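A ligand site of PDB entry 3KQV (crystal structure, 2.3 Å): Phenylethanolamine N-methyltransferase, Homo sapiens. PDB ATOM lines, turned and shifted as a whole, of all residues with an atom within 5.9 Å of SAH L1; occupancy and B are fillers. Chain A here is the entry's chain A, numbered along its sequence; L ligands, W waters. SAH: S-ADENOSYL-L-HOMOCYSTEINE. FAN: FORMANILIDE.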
ATOM      1  N   TYR A  27      24.334  -5.463  -6.159  1.00  0.00           N
ATOM      2  CA  TYR A  27      24.132  -6.901  -6.025  1.00  0.00           C
ATOM      3  C   TYR A  27      22.943  -7.413  -6.826  1.00  0.00           C
ATOM      4  O   TYR A  27      22.762  -8.613  -6.968  1.00  0.00           O
ATOM      5  CB  TYR A  27      24.012  -7.318  -4.557  1.00  0.00           C
ATOM      6  CG  TYR A  27      25.360  -7.558  -3.912  1.00  0.00           C
ATOM      7  CD1 TYR A  27      25.979  -6.581  -3.148  1.00  0.00           C
ATOM      8  CD2 TYR A  27      26.031  -8.756  -4.112  1.00  0.00           C
ATOM      9  CE1 TYR A  27      27.211  -6.798  -2.581  1.00  0.00           C
ATOM     10  CE2 TYR A  27      27.268  -8.992  -3.550  1.00  0.00           C
ATOM     11  CZ  TYR A  27      27.851  -8.005  -2.781  1.00  0.00           C
ATOM     12  OH  TYR A  27      29.094  -8.236  -2.231  1.00  0.00           O
ATOM     13  N   PHE A  30      24.306  -9.247  -9.684  1.00  0.00           N
ATOM     14  CA  PHE A  30      25.177 -10.340  -9.280  1.00  0.00           C
ATOM     15  C   PHE A  30      24.754 -11.645  -9.954  1.00  0.00           C
ATOM     16  O   PHE A  30      23.633 -12.115  -9.740  1.00  0.00           O
ATOM     17  CB  PHE A  30      25.130 -10.484  -7.752  1.00  0.00           C
ATOM     18  CG  PHE A  30      26.026 -11.552  -7.189  1.00  0.00           C
ATOM     19  CD1 PHE A  30      27.219 -11.222  -6.575  1.00  0.00           C
ATOM     20  CD2 PHE A  30      25.650 -12.889  -7.237  1.00  0.00           C
ATOM     21  CE1 PHE A  30      28.046 -12.203  -6.044  1.00  0.00           C
ATOM     22  CE2 PHE A  30      26.460 -13.878  -6.700  1.00  0.00           C
ATOM     23  CZ  PHE A  30      27.659 -13.528  -6.108  1.00  0.00           C
ATOM     24  N   TYR A  35      30.103 -15.804 -10.657  1.00  0.00           N
ATOM     25  CA  TYR A  35      30.852 -15.825  -9.396  1.00  0.00           C
ATOM     26  C   TYR A  35      31.529 -17.176  -9.151  1.00  0.00           C
ATOM     27  O   TYR A  35      32.695 -17.234  -8.781  1.00  0.00           O
ATOM     28  CB  TYR A  35      29.937 -15.472  -8.223  1.00  0.00           C
ATOM     29  CG  TYR A  35      30.621 -15.537  -6.875  1.00  0.00           C
ATOM     30  CD1 TYR A  35      31.495 -14.532  -6.470  1.00  0.00           C
ATOM     31  CD2 TYR A  35      30.388 -16.589  -5.998  1.00  0.00           C
ATOM     32  CE1 TYR A  35      32.135 -14.587  -5.234  1.00  0.00           C
ATOM     33  CE2 TYR A  35      31.010 -16.651  -4.756  1.00  0.00           C
ATOM     34  CZ  TYR A  35      31.884 -15.647  -4.384  1.00  0.00           C
ATOM     35  OH  TYR A  35      32.505 -15.693  -3.160  1.00  0.00           O
ATOM     36  N   TYR A  40      35.660 -20.532  -8.120  1.00  0.00           N
ATOM     37  CA  TYR A  40      35.612 -21.943  -7.750  1.00  0.00           C
ATOM     38  C   TYR A  40      35.818 -22.902  -8.910  1.00  0.00           C
ATOM     39  O   TYR A  40      35.607 -24.109  -8.765  1.00  0.00           O
ATOM     40  CB  TYR A  40      34.333 -22.221  -6.949  1.00  0.00           C
ATOM     41  CG  TYR A  40      34.324 -21.425  -5.671  1.00  0.00           C
ATOM     42  CD1 TYR A  40      33.664 -20.212  -5.583  1.00  0.00           C
ATOM     43  CD2 TYR A  40      35.047 -21.863  -4.559  1.00  0.00           C
ATOM     44  CE1 TYR A  40      33.683 -19.472  -4.414  1.00  0.00           C
ATOM     45  CE2 TYR A  40      35.073 -21.134  -3.384  1.00  0.00           C
ATOM     46  CZ  TYR A  40      34.389 -19.942  -3.323  1.00  0.00           C
ATOM     47  OH  TYR A  40      34.414 -19.213  -2.148  1.00  0.00           O
ATOM     48  N   LYS A  57      41.900 -22.710   2.540  1.00  0.00           N
ATOM     49  CA  LYS A  57      40.624 -22.460   3.201  1.00  0.00           C
ATOM     50  C   LYS A  57      40.063 -23.721   3.851  1.00  0.00           C
ATOM     51  O   LYS A  57      39.698 -23.723   5.034  1.00  0.00           O
ATOM     52  CB  LYS A  57      39.607 -21.874   2.219  1.00  0.00           C
ATOM     53  CG  LYS A  57      40.004 -20.497   1.681  1.00  0.00           C
ATOM     54  CD  LYS A  57      38.845 -19.776   1.016  1.00  0.00           C
ATOM     55  CE  LYS A  57      38.346 -20.513  -0.221  1.00  0.00           C
ATOM     56  NZ  LYS A  57      37.327 -19.713  -0.943  1.00  0.00           N
ATOM     57  N   ASP A  77      25.223 -20.342   8.653  1.00  0.00           N
ATOM     58  CA  ASP A  77      26.163 -19.826   7.676  1.00  0.00           C
ATOM     59  C   ASP A  77      25.660 -18.492   7.144  1.00  0.00           C
ATOM     60  O   ASP A  77      24.551 -18.412   6.610  1.00  0.00           O
ATOM     61  CB  ASP A  77      26.341 -20.827   6.520  1.00  0.00           C
ATOM     62  CG  ASP A  77      27.403 -20.379   5.523  1.00  0.00           C
ATOM     63  OD1 ASP A  77      28.350 -19.692   5.941  1.00  0.00           O
ATOM     64  OD2 ASP A  77      27.273 -20.697   4.322  1.00  0.00           O
ATOM     65  N   ILE A  78      26.462 -17.444   7.300  1.00  0.00           N
ATOM     66  CA  ILE A  78      26.092 -16.065   6.962  1.00  0.00           C
ATOM     67  C   ILE A  78      26.576 -15.625   5.583  1.00  0.00           C
ATOM     68  O   ILE A  78      27.783 -15.575   5.337  1.00  0.00           O
ATOM     69  CB  ILE A  78      26.678 -15.063   7.975  1.00  0.00           C
ATOM     70  CG1 ILE A  78      26.271 -15.412   9.413  1.00  0.00           C
ATOM     71  CG2 ILE A  78      26.268 -13.649   7.627  1.00  0.00           C
ATOM     72  CD1 ILE A  78      24.782 -15.365   9.644  1.00  0.00           C
ATOM     73  N   GLY A  79      25.653 -15.278   4.696  1.00  0.00           N
ATOM     74  CA  GLY A  79      26.009 -14.893   3.342  1.00  0.00           C
ATOM     75  C   GLY A  79      26.645 -16.040   2.570  1.00  0.00           C
ATOM     76  O   GLY A  79      27.753 -15.898   2.029  1.00  0.00           O
ATOM     77  N   SER A  80      25.939 -17.162   2.502  1.00  0.00           N
ATOM     78  CA  SER A  80      26.451 -18.362   1.863  1.00  0.00           C
ATOM     79  C   SER A  80      26.743 -18.163   0.382  1.00  0.00           C
ATOM     80  O   SER A  80      27.570 -18.869  -0.197  1.00  0.00           O
ATOM     81  CB  SER A  80      25.432 -19.506   2.004  1.00  0.00           C
ATOM     82  OG  SER A  80      24.990 -19.629   3.342  1.00  0.00           O
ATOM     83  N   GLY A  81      26.065 -17.202  -0.228  1.00  0.00           N
ATOM     84  CA  GLY A  81      26.098 -17.096  -1.679  1.00  0.00           C
ATOM     85  C   GLY A  81      25.677 -18.416  -2.301  1.00  0.00           C
ATOM     86  O   GLY A  81      24.796 -19.094  -1.775  1.00  0.00           O
ATOM     87  N   PRO A  82      26.316 -18.789  -3.414  1.00  0.00           N
ATOM     88  CA  PRO A  82      25.989 -20.039  -4.108  1.00  0.00           C
ATOM     89  C   PRO A  82      26.934 -21.186  -3.745  1.00  0.00           C
ATOM     90  O   PRO A  82      27.029 -22.148  -4.494  1.00  0.00           O
ATOM     91  CB  PRO A  82      26.210 -19.688  -5.587  1.00  0.00           C
ATOM     92  CG  PRO A  82      26.979 -18.354  -5.587  1.00  0.00           C
ATOM     93  CD  PRO A  82      27.303 -18.013  -4.167  1.00  0.00           C
ATOM     94  N   THR A  83      27.638 -21.072  -2.617  1.00  0.00           N
ATOM     95  CA  THR A  83      28.684 -22.057  -2.302  1.00  0.00           C
ATOM     96  C   THR A  83      28.362 -22.871  -1.037  1.00  0.00           C
ATOM     97  O   THR A  83      27.631 -22.398  -0.165  1.00  0.00           O
ATOM     98  CB  THR A  83      30.071 -21.381  -2.153  1.00  0.00           C
ATOM     99  OG1 THR A  83      30.120 -20.638  -0.931  1.00  0.00           O
ATOM    100  CG2 THR A  83      30.333 -20.425  -3.335  1.00  0.00           C
ATOM    101  N   TYR A  85      31.144 -25.187   0.183  1.00  0.00           N
ATOM    102  CA  TYR A  85      32.439 -25.730   0.633  1.00  0.00           C
ATOM    103  C   TYR A  85      32.714 -25.333   2.073  1.00  0.00           C
ATOM    104  O   TYR A  85      33.398 -26.057   2.799  1.00  0.00           O
ATOM    105  CB  TYR A  85      33.586 -25.217  -0.246  1.00  0.00           C
ATOM    106  CG  TYR A  85      33.889 -23.750   0.023  1.00  0.00           C
ATOM    107  CD1 TYR A  85      34.843 -23.363   0.947  1.00  0.00           C
ATOM    108  CD2 TYR A  85      33.163 -22.751  -0.615  1.00  0.00           C
ATOM    109  CE1 TYR A  85      35.105 -22.026   1.211  1.00  0.00           C
ATOM    110  CE2 TYR A  85      33.408 -21.414  -0.366  1.00  0.00           C
ATOM    111  CZ  TYR A  85      34.373 -21.064   0.547  1.00  0.00           C
ATOM    112  OH  TYR A  85      34.612 -19.740   0.796  1.00  0.00           O
ATOM    113  N   GLN A  86      32.202 -24.181   2.472  1.00  0.00           N
ATOM    114  CA  GLN A  86      32.492 -23.638   3.798  1.00  0.00           C
ATOM    115  C   GLN A  86      31.821 -24.413   4.923  1.00  0.00           C
ATOM    116  O   GLN A  86      32.038 -24.115   6.095  1.00  0.00           O
ATOM    117  CB  GLN A  86      32.095 -22.152   3.876  1.00  0.00           C
ATOM    118  CG  GLN A  86      30.596 -21.882   3.786  1.00  0.00           C
ATOM    119  CD  GLN A  86      30.120 -21.599   2.375  1.00  0.00           C
ATOM    120  OE1 GLN A  86      30.745 -22.016   1.394  1.00  0.00           O
ATOM    121  NE2 GLN A  86      29.017 -20.870   2.250  1.00  0.00           N
ATOM    122  N   ASP A 101      21.335 -16.115   2.419  1.00  0.00           N
ATOM    123  CA  ASP A 101      21.869 -15.092   1.529  1.00  0.00           C
ATOM    124  C   ASP A 101      20.865 -14.001   1.226  1.00  0.00           C
ATOM    125  O   ASP A 101      19.649 -14.211   1.272  1.00  0.00           O
ATOM    126  CB  ASP A 101      22.387 -15.681   0.222  1.00  0.00           C
ATOM    127  CG  ASP A 101      23.402 -14.782  -0.445  1.00  0.00           C
ATOM    128  OD1 ASP A 101      24.505 -14.646   0.118  1.00  0.00           O
ATOM    129  OD2 ASP A 101      23.080 -14.191  -1.504  1.00  0.00           O
ATOM    130  N   PHE A 102      21.407 -12.837   0.886  1.00  0.00           N
ATOM    131  CA  PHE A 102      20.614 -11.670   0.527  1.00  0.00           C
ATOM    132  C   PHE A 102      19.847 -11.893  -0.769  1.00  0.00           C
ATOM    133  O   PHE A 102      18.701 -11.452  -0.915  1.00  0.00           O
ATOM    134  CB  PHE A 102      21.531 -10.444   0.412  1.00  0.00           C
ATOM    135  CG  PHE A 102      20.804  -9.148   0.157  1.00  0.00           C
ATOM    136  CD1 PHE A 102      20.078  -8.539   1.161  1.00  0.00           C
ATOM    137  CD2 PHE A 102      20.874  -8.533  -1.078  1.00  0.00           C
ATOM    138  CE1 PHE A 102      19.413  -7.351   0.927  1.00  0.00           C
ATOM    139  CE2 PHE A 102      20.223  -7.337  -1.328  1.00  0.00           C
ATOM    140  CZ  PHE A 102      19.486  -6.746  -0.312  1.00  0.00           C
ATOM    141  N   LEU A 103      20.465 -12.605  -1.711  1.00  0.00           N
ATOM    142  CA  LEU A 103      19.888 -12.749  -3.053  1.00  0.00           C
ATOM    143  C   LEU A 103      19.090 -14.028  -3.263  1.00  0.00           C
ATOM    144  O   LEU A 103      19.530 -15.126  -2.894  1.00  0.00           O
ATOM    145  CB  LEU A 103      20.983 -12.627  -4.122  1.00  0.00           C
ATOM    146  CG  LEU A 103      21.685 -11.271  -4.188  1.00  0.00           C
ATOM    147  CD1 LEU A 103      22.775 -11.287  -5.234  1.00  0.00           C
ATOM    148  CD2 LEU A 103      20.658 -10.169  -4.479  1.00  0.00           C
ATOM    149  N   ASN A 106      20.891 -16.695  -5.441  1.00  0.00           N
ATOM    150  CA  ASN A 106      21.852 -17.523  -4.720  1.00  0.00           C
ATOM    151  C   ASN A 106      21.160 -18.622  -3.941  1.00  0.00           C
ATOM    152  O   ASN A 106      21.630 -19.762  -3.912  1.00  0.00           O
ATOM    153  CB  ASN A 106      22.723 -16.701  -3.773  1.00  0.00           C
ATOM    154  CG  ASN A 106      23.879 -16.030  -4.485  1.00  0.00           C
ATOM    155  OD1 ASN A 106      24.421 -15.034  -4.005  1.00  0.00           O
ATOM    156  ND2 ASN A 106      24.270 -16.583  -5.632  1.00  0.00           N
ATOM    157  N   ILE A 157      18.577 -12.963   4.268  1.00  0.00           N
ATOM    158  CA  ILE A 157      19.296 -12.299   5.342  1.00  0.00           C
ATOM    159  C   ILE A 157      19.820 -10.958   4.865  1.00  0.00           C
ATOM    160  O   ILE A 157      20.105 -10.784   3.680  1.00  0.00           O
ATOM    161  CB  ILE A 157      20.455 -13.174   5.870  1.00  0.00           C
ATOM    162  CG1 ILE A 157      21.047 -12.575   7.153  1.00  0.00           C
ATOM    163  CG2 ILE A 157      21.519 -13.351   4.796  1.00  0.00           C
ATOM    164  CD1 ILE A 157      22.048 -13.485   7.864  1.00  0.00           C
ATOM    165  N   ASP A 158      19.911 -10.002   5.775  1.00  0.00           N
ATOM    166  CA  ASP A 158      20.538  -8.720   5.486  1.00  0.00           C
ATOM    167  C   ASP A 158      21.325  -8.273   6.702  1.00  0.00           C
ATOM    168  O   ASP A 158      20.755  -7.797   7.681  1.00  0.00           O
ATOM    169  CB  ASP A 158      19.499  -7.662   5.114  1.00  0.00           C
ATOM    170  CG  ASP A 158      20.121  -6.315   4.816  1.00  0.00           C
ATOM    171  OD1 ASP A 158      21.360  -6.173   4.947  1.00  0.00           O
ATOM    172  OD2 ASP A 158      19.372  -5.382   4.452  1.00  0.00           O
ATOM    173  N   VAL A 159      22.652  -8.426   6.633  1.00  0.00           N
ATOM    174  CA  VAL A 159      23.509  -8.110   7.774  1.00  0.00           C
ATOM    175  C   VAL A 159      23.485  -6.622   8.132  1.00  0.00           C
ATOM    176  O   VAL A 159      23.985  -6.230   9.187  1.00  0.00           O
ATOM    177  CB  VAL A 159      24.947  -8.574   7.515  1.00  0.00           C
ATOM    178  CG1 VAL A 159      24.980 -10.085   7.281  1.00  0.00           C
ATOM    179  CG2 VAL A 159      25.530  -7.829   6.334  1.00  0.00           C
ATOM    180  N   HIS A 160      22.924  -5.798   7.260  1.00  0.00           N
ATOM    181  CA  HIS A 160      22.795  -4.372   7.542  1.00  0.00           C
ATOM    182  C   HIS A 160      21.704  -4.105   8.577  1.00  0.00           C
ATOM    183  O   HIS A 160      21.674  -3.045   9.205  1.00  0.00           O
ATOM    184  CB  HIS A 160      22.476  -3.578   6.274  1.00  0.00           C
ATOM    185  CG  HIS A 160      23.544  -3.654   5.227  1.00  0.00           C
ATOM    186  ND1 HIS A 160      24.890  -3.598   5.528  1.00  0.00           N
ATOM    187  CD2 HIS A 160      23.476  -3.771   3.880  1.00  0.00           C
ATOM    188  CE1 HIS A 160      25.596  -3.682   4.415  1.00  0.00           C
ATOM    189  NE2 HIS A 160      24.758  -3.782   3.402  1.00  0.00           N
ATOM    190  N   SER A 180      31.047 -17.575   8.356  1.00  0.00           N
ATOM    191  CA  SER A 180      30.804 -16.597   7.308  1.00  0.00           C
ATOM    192  C   SER A 180      32.041 -16.347   6.455  1.00  0.00           C
ATOM    193  O   SER A 180      33.102 -16.003   6.972  1.00  0.00           O
ATOM    194  CB  SER A 180      30.296 -15.268   7.880  1.00  0.00           C
ATOM    195  OG  SER A 180      29.945 -14.395   6.827  1.00  0.00           O
ATOM    196  N   ALA A 181      31.882 -16.513   5.149  1.00  0.00           N
ATOM    197  CA  ALA A 181      33.015 -16.419   4.247  1.00  0.00           C
ATOM    198  C   ALA A 181      32.791 -15.373   3.169  1.00  0.00           C
ATOM    199  O   ALA A 181      31.894 -15.509   2.330  1.00  0.00           O
ATOM    200  CB  ALA A 181      33.289 -17.786   3.615  1.00  0.00           C
ATOM    201  N   PHE A 182      33.591 -14.313   3.208  1.00  0.00           N
ATOM    202  CA  PHE A 182      33.594 -13.297   2.159  1.00  0.00           C
ATOM    203  C   PHE A 182      32.283 -12.522   2.043  1.00  0.00           C
ATOM    204  O   PHE A 182      31.909 -12.080   0.958  1.00  0.00           O
ATOM    205  CB  PHE A 182      33.914 -13.926   0.798  1.00  0.00           C
ATOM    206  CG  PHE A 182      35.217 -14.670   0.768  1.00  0.00           C
ATOM    207  CD1 PHE A 182      35.229 -16.060   0.763  1.00  0.00           C
ATOM    208  CD2 PHE A 182      36.426 -13.992   0.740  1.00  0.00           C
ATOM    209  CE1 PHE A 182      36.427 -16.755   0.721  1.00  0.00           C
ATOM    210  CE2 PHE A 182      37.628 -14.688   0.707  1.00  0.00           C
ATOM    211  CZ  PHE A 182      37.625 -16.071   0.699  1.00  0.00           C
ATOM    212  N   CYS A 183      31.578 -12.352   3.160  1.00  0.00           N
ATOM    213  CA  CYS A 183      30.343 -11.572   3.133  1.00  0.00           C
ATOM    214  C   CYS A 183      30.544 -10.127   3.596  1.00  0.00           C
ATOM    215  O   CYS A 183      30.390  -9.192   2.811  1.00  0.00           O
ATOM    216  CB  CYS A 183      29.263 -12.260   3.975  1.00  0.00           C
ATOM    217  SG  CYS A 183      27.650 -11.415   3.913  1.00  0.00           S
ATOM    218  N   ALA A 186      32.544  -7.584   1.799  1.00  0.00           N
ATOM    219  CA  ALA A 186      31.976  -7.489   0.461  1.00  0.00           C
ATOM    220  C   ALA A 186      30.634  -6.760   0.395  1.00  0.00           C
ATOM    221  O   ALA A 186      30.120  -6.486  -0.693  1.00  0.00           O
ATOM    222  CB  ALA A 186      31.848  -8.888  -0.158  1.00  0.00           C
ATOM    223  N   VAL A 187      30.055  -6.446   1.548  1.00  0.00           N
ATOM    224  CA  VAL A 187      28.781  -5.730   1.593  1.00  0.00           C
ATOM    225  C   VAL A 187      28.863  -4.413   2.372  1.00  0.00           C
ATOM    226  O   VAL A 187      27.851  -3.771   2.623  1.00  0.00           O
ATOM    227  CB  VAL A 187      27.639  -6.618   2.173  1.00  0.00           C
ATOM    228  CG1 VAL A 187      27.585  -7.946   1.458  1.00  0.00           C
ATOM    229  CG2 VAL A 187      27.836  -6.834   3.672  1.00  0.00           C
ATOM    230  N   TYR A 222      35.364  -6.726  -6.821  1.00  0.00           N
ATOM    231  CA  TYR A 222      35.373  -7.991  -7.542  1.00  0.00           C
ATOM    232  C   TYR A 222      34.188  -8.038  -8.484  1.00  0.00           C
ATOM    233  O   TYR A 222      33.270  -7.218  -8.376  1.00  0.00           O
ATOM    234  CB  TYR A 222      35.365  -9.188  -6.578  1.00  0.00           C
ATOM    235  CG  TYR A 222      34.051  -9.453  -5.893  1.00  0.00           C
ATOM    236  CD1 TYR A 222      33.248 -10.508  -6.281  1.00  0.00           C
ATOM    237  CD2 TYR A 222      33.618  -8.647  -4.837  1.00  0.00           C
ATOM    238  CE1 TYR A 222      32.046 -10.767  -5.654  1.00  0.00           C
ATOM    239  CE2 TYR A 222      32.412  -8.903  -4.186  1.00  0.00           C
ATOM    240  CZ  TYR A 222      31.633  -9.963  -4.608  1.00  0.00           C
ATOM    241  OH  TYR A 222      30.435 -10.248  -3.998  1.00  0.00           O
HETATM  242  N   SAH L   1      30.040 -17.087   1.167  1.00  0.00           N
HETATM  243  CA  SAH L   1      30.336 -17.460  -0.206  1.00  0.00           C
HETATM  244  CB  SAH L   1      30.010 -16.330  -1.192  1.00  0.00           C
HETATM  245  CG  SAH L   1      30.423 -14.961  -0.635  1.00  0.00           C
HETATM  246  SD  SAH L   1      29.953 -13.691  -1.865  1.00  0.00           S
HETATM  247  C   SAH L   1      31.809 -17.860  -0.359  1.00  0.00           C
HETATM  248  O   SAH L   1      32.430 -18.310   0.552  1.00  0.00           O
HETATM  249  OXT SAH L   1      32.371 -17.839  -1.634  1.00  0.00           O
HETATM  250  C5' SAH L   1      29.215 -12.285  -0.971  1.00  0.00           C
HETATM  251  C4' SAH L   1      27.751 -12.625  -0.653  1.00  0.00           C
HETATM  252  O4' SAH L   1      27.161 -11.630   0.238  1.00  0.00           O
HETATM  253  C3' SAH L   1      26.868 -12.665  -1.912  1.00  0.00           C
HETATM  254  O3' SAH L   1      26.253 -13.918  -1.997  1.00  0.00           O
HETATM  255  C2' SAH L   1      25.846 -11.599  -1.638  1.00  0.00           C
HETATM  256  O2' SAH L   1      24.615 -11.888  -2.250  1.00  0.00           O
HETATM  257  C1' SAH L   1      25.741 -11.636  -0.122  1.00  0.00           C
HETATM  258  N9  SAH L   1      25.165 -10.367   0.293  1.00  0.00           N
HETATM  259  C8  SAH L   1      25.034  -9.161  -0.577  1.00  0.00           C
HETATM  260  N7  SAH L   1      24.411  -8.115   0.216  1.00  0.00           N
HETATM  261  C5  SAH L   1      24.150  -8.656   1.569  1.00  0.00           C
HETATM  262  C6  SAH L   1      23.539  -8.033   2.779  1.00  0.00           C
HETATM  263  N6  SAH L   1      23.082  -6.656   2.730  1.00  0.00           N
HETATM  264  N1  SAH L   1      23.411  -8.824   4.008  1.00  0.00           N
HETATM  265  C2  SAH L   1      23.881 -10.247   4.043  1.00  0.00           C
HETATM  266  N3  SAH L   1      24.498 -10.857   2.832  1.00  0.00           N
HETATM  267  C4  SAH L   1      24.626 -10.066   1.603  1.00  0.00           C
HETATM  268  C1  FAN L   2      39.030 -15.185  -2.972  1.00  0.00           C
HETATM  269  C2  FAN L   2      37.950 -14.262  -3.074  1.00  0.00           C
HETATM  270  C3  FAN L   2      36.592 -14.739  -2.990  1.00  0.00           C
HETATM  271  C4  FAN L   2      36.368 -16.134  -2.806  1.00  0.00           C
HETATM  272  C5  FAN L   2      37.456 -17.053  -2.708  1.00  0.00           C
HETATM  273  C6  FAN L   2      38.796 -16.591  -2.797  1.00  0.00           C
HETATM  274  C7  FAN L   2      35.382 -12.447  -2.621  1.00  0.00           C
HETATM  275  N1  FAN L   2      35.433 -13.841  -3.085  1.00  0.00           N
HETATM  276  O1  FAN L   2      35.821 -11.534  -3.235  1.00  0.00           O
HETATM  277  O   HOH W   1      23.176  -4.742   0.311  1.00  0.00           O
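The side-chain hydroxyl of Tyr 35 is in hydrogen-bond range of a nitrogen (N1) of FAN L2 (3.5 Å).
The side-chain hydroxyl (OH) of Tyr 40 is in hydrogen-bond range of an oxygen (OXT) of SAH L1 (2.5 Å).
The side-chain amide oxygen of Asn 106 lies within hydrogen-bond range of an oxygen (O3') of SAH L1, 2.9 Å away.
An oxygen (O3') of SAH L1 is in hydrogen-bond range of the side-chain carboxylate (OD1) of Asp 101.
N6 of SAH L1 sits at hydrogen-bond distance from OD1 of Asp 158.
N of Val 159 sits at hydrogen-bond distance from N1 of SAH L1 (2.8 Å).
N of SAH L1 lies within hydrogen-bond range of O of Ala 181, at 2.7 Å.
A ring nitrogen (NE2) of His 160 lies close to a nitrogen (N6) of SAH L1, at 3.4 Å.
An oxygen (OXT) of SAH L1 lies within hydrogen-bond range of the side-chain hydroxyl (OH) of Tyr 35, 2.6 Å away.
The backbone carbonyl oxygen of Gly 79 is in hydrogen-bond range of a nitrogen (N) of SAH L1.
The side-chain hydroxyl (OH) of Tyr 85 sits at hydrogen-bond distance from an oxygen (O) of SAH L1 (2.6 Å).
The backbone carbonyl oxygen of Ser 80 lies close to a nitrogen (N) of SAH L1 (3.3 Å).
The side-chain sulfur (SG) of Cys 183 sits at hydrogen-bond distance from a nitrogen (N3) of SAH L1, at 3.4 Å.
OD2 of Asp 101 sits close to OD1 of Asn 106.
OH of Tyr 85 is in hydrogen-bond range of NZ of Lys 57.
The backbone NH of Ile 157 is in hydrogen-bond range of the backbone carbonyl oxygen of Asp 101 (3.4 Å).
The side-chain hydroxyl (OH) of Tyr 85 is in hydrogen-bond range of the side-chain hydroxyl (OH) of Tyr 40 (3.0 Å).
The side-chain carboxylate (OD1) of Asp 158 sits at hydrogen-bond distance from the backbone NH (N) of His 160 (2.8 Å).
The side-chain carboxylate (OD1) of Asp 101 sits at hydrogen-bond distance from the backbone NH (N) of Gly 81, at 3.0 Å.
The side-chain hydroxyl of Ser 80 is in hydrogen-bond range of the side-chain carboxylate of Asp 77 (2.7 Å).
The backbone carbonyl oxygen (O) of Ser 80 is in hydrogen-bond range of the side-chain amide nitrogen (NE2) of Gln 86.
The backbone carbonyl oxygen (O) of Phe 182 sits close to a sulfur (SD) of SAH L1 (3.8 Å).
Residues that only touch SAH L1: Gly 81, Thr 83, Phe 102, Val 187, Tyr 27, Leu 103, Ile 157 and Tyr 222.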
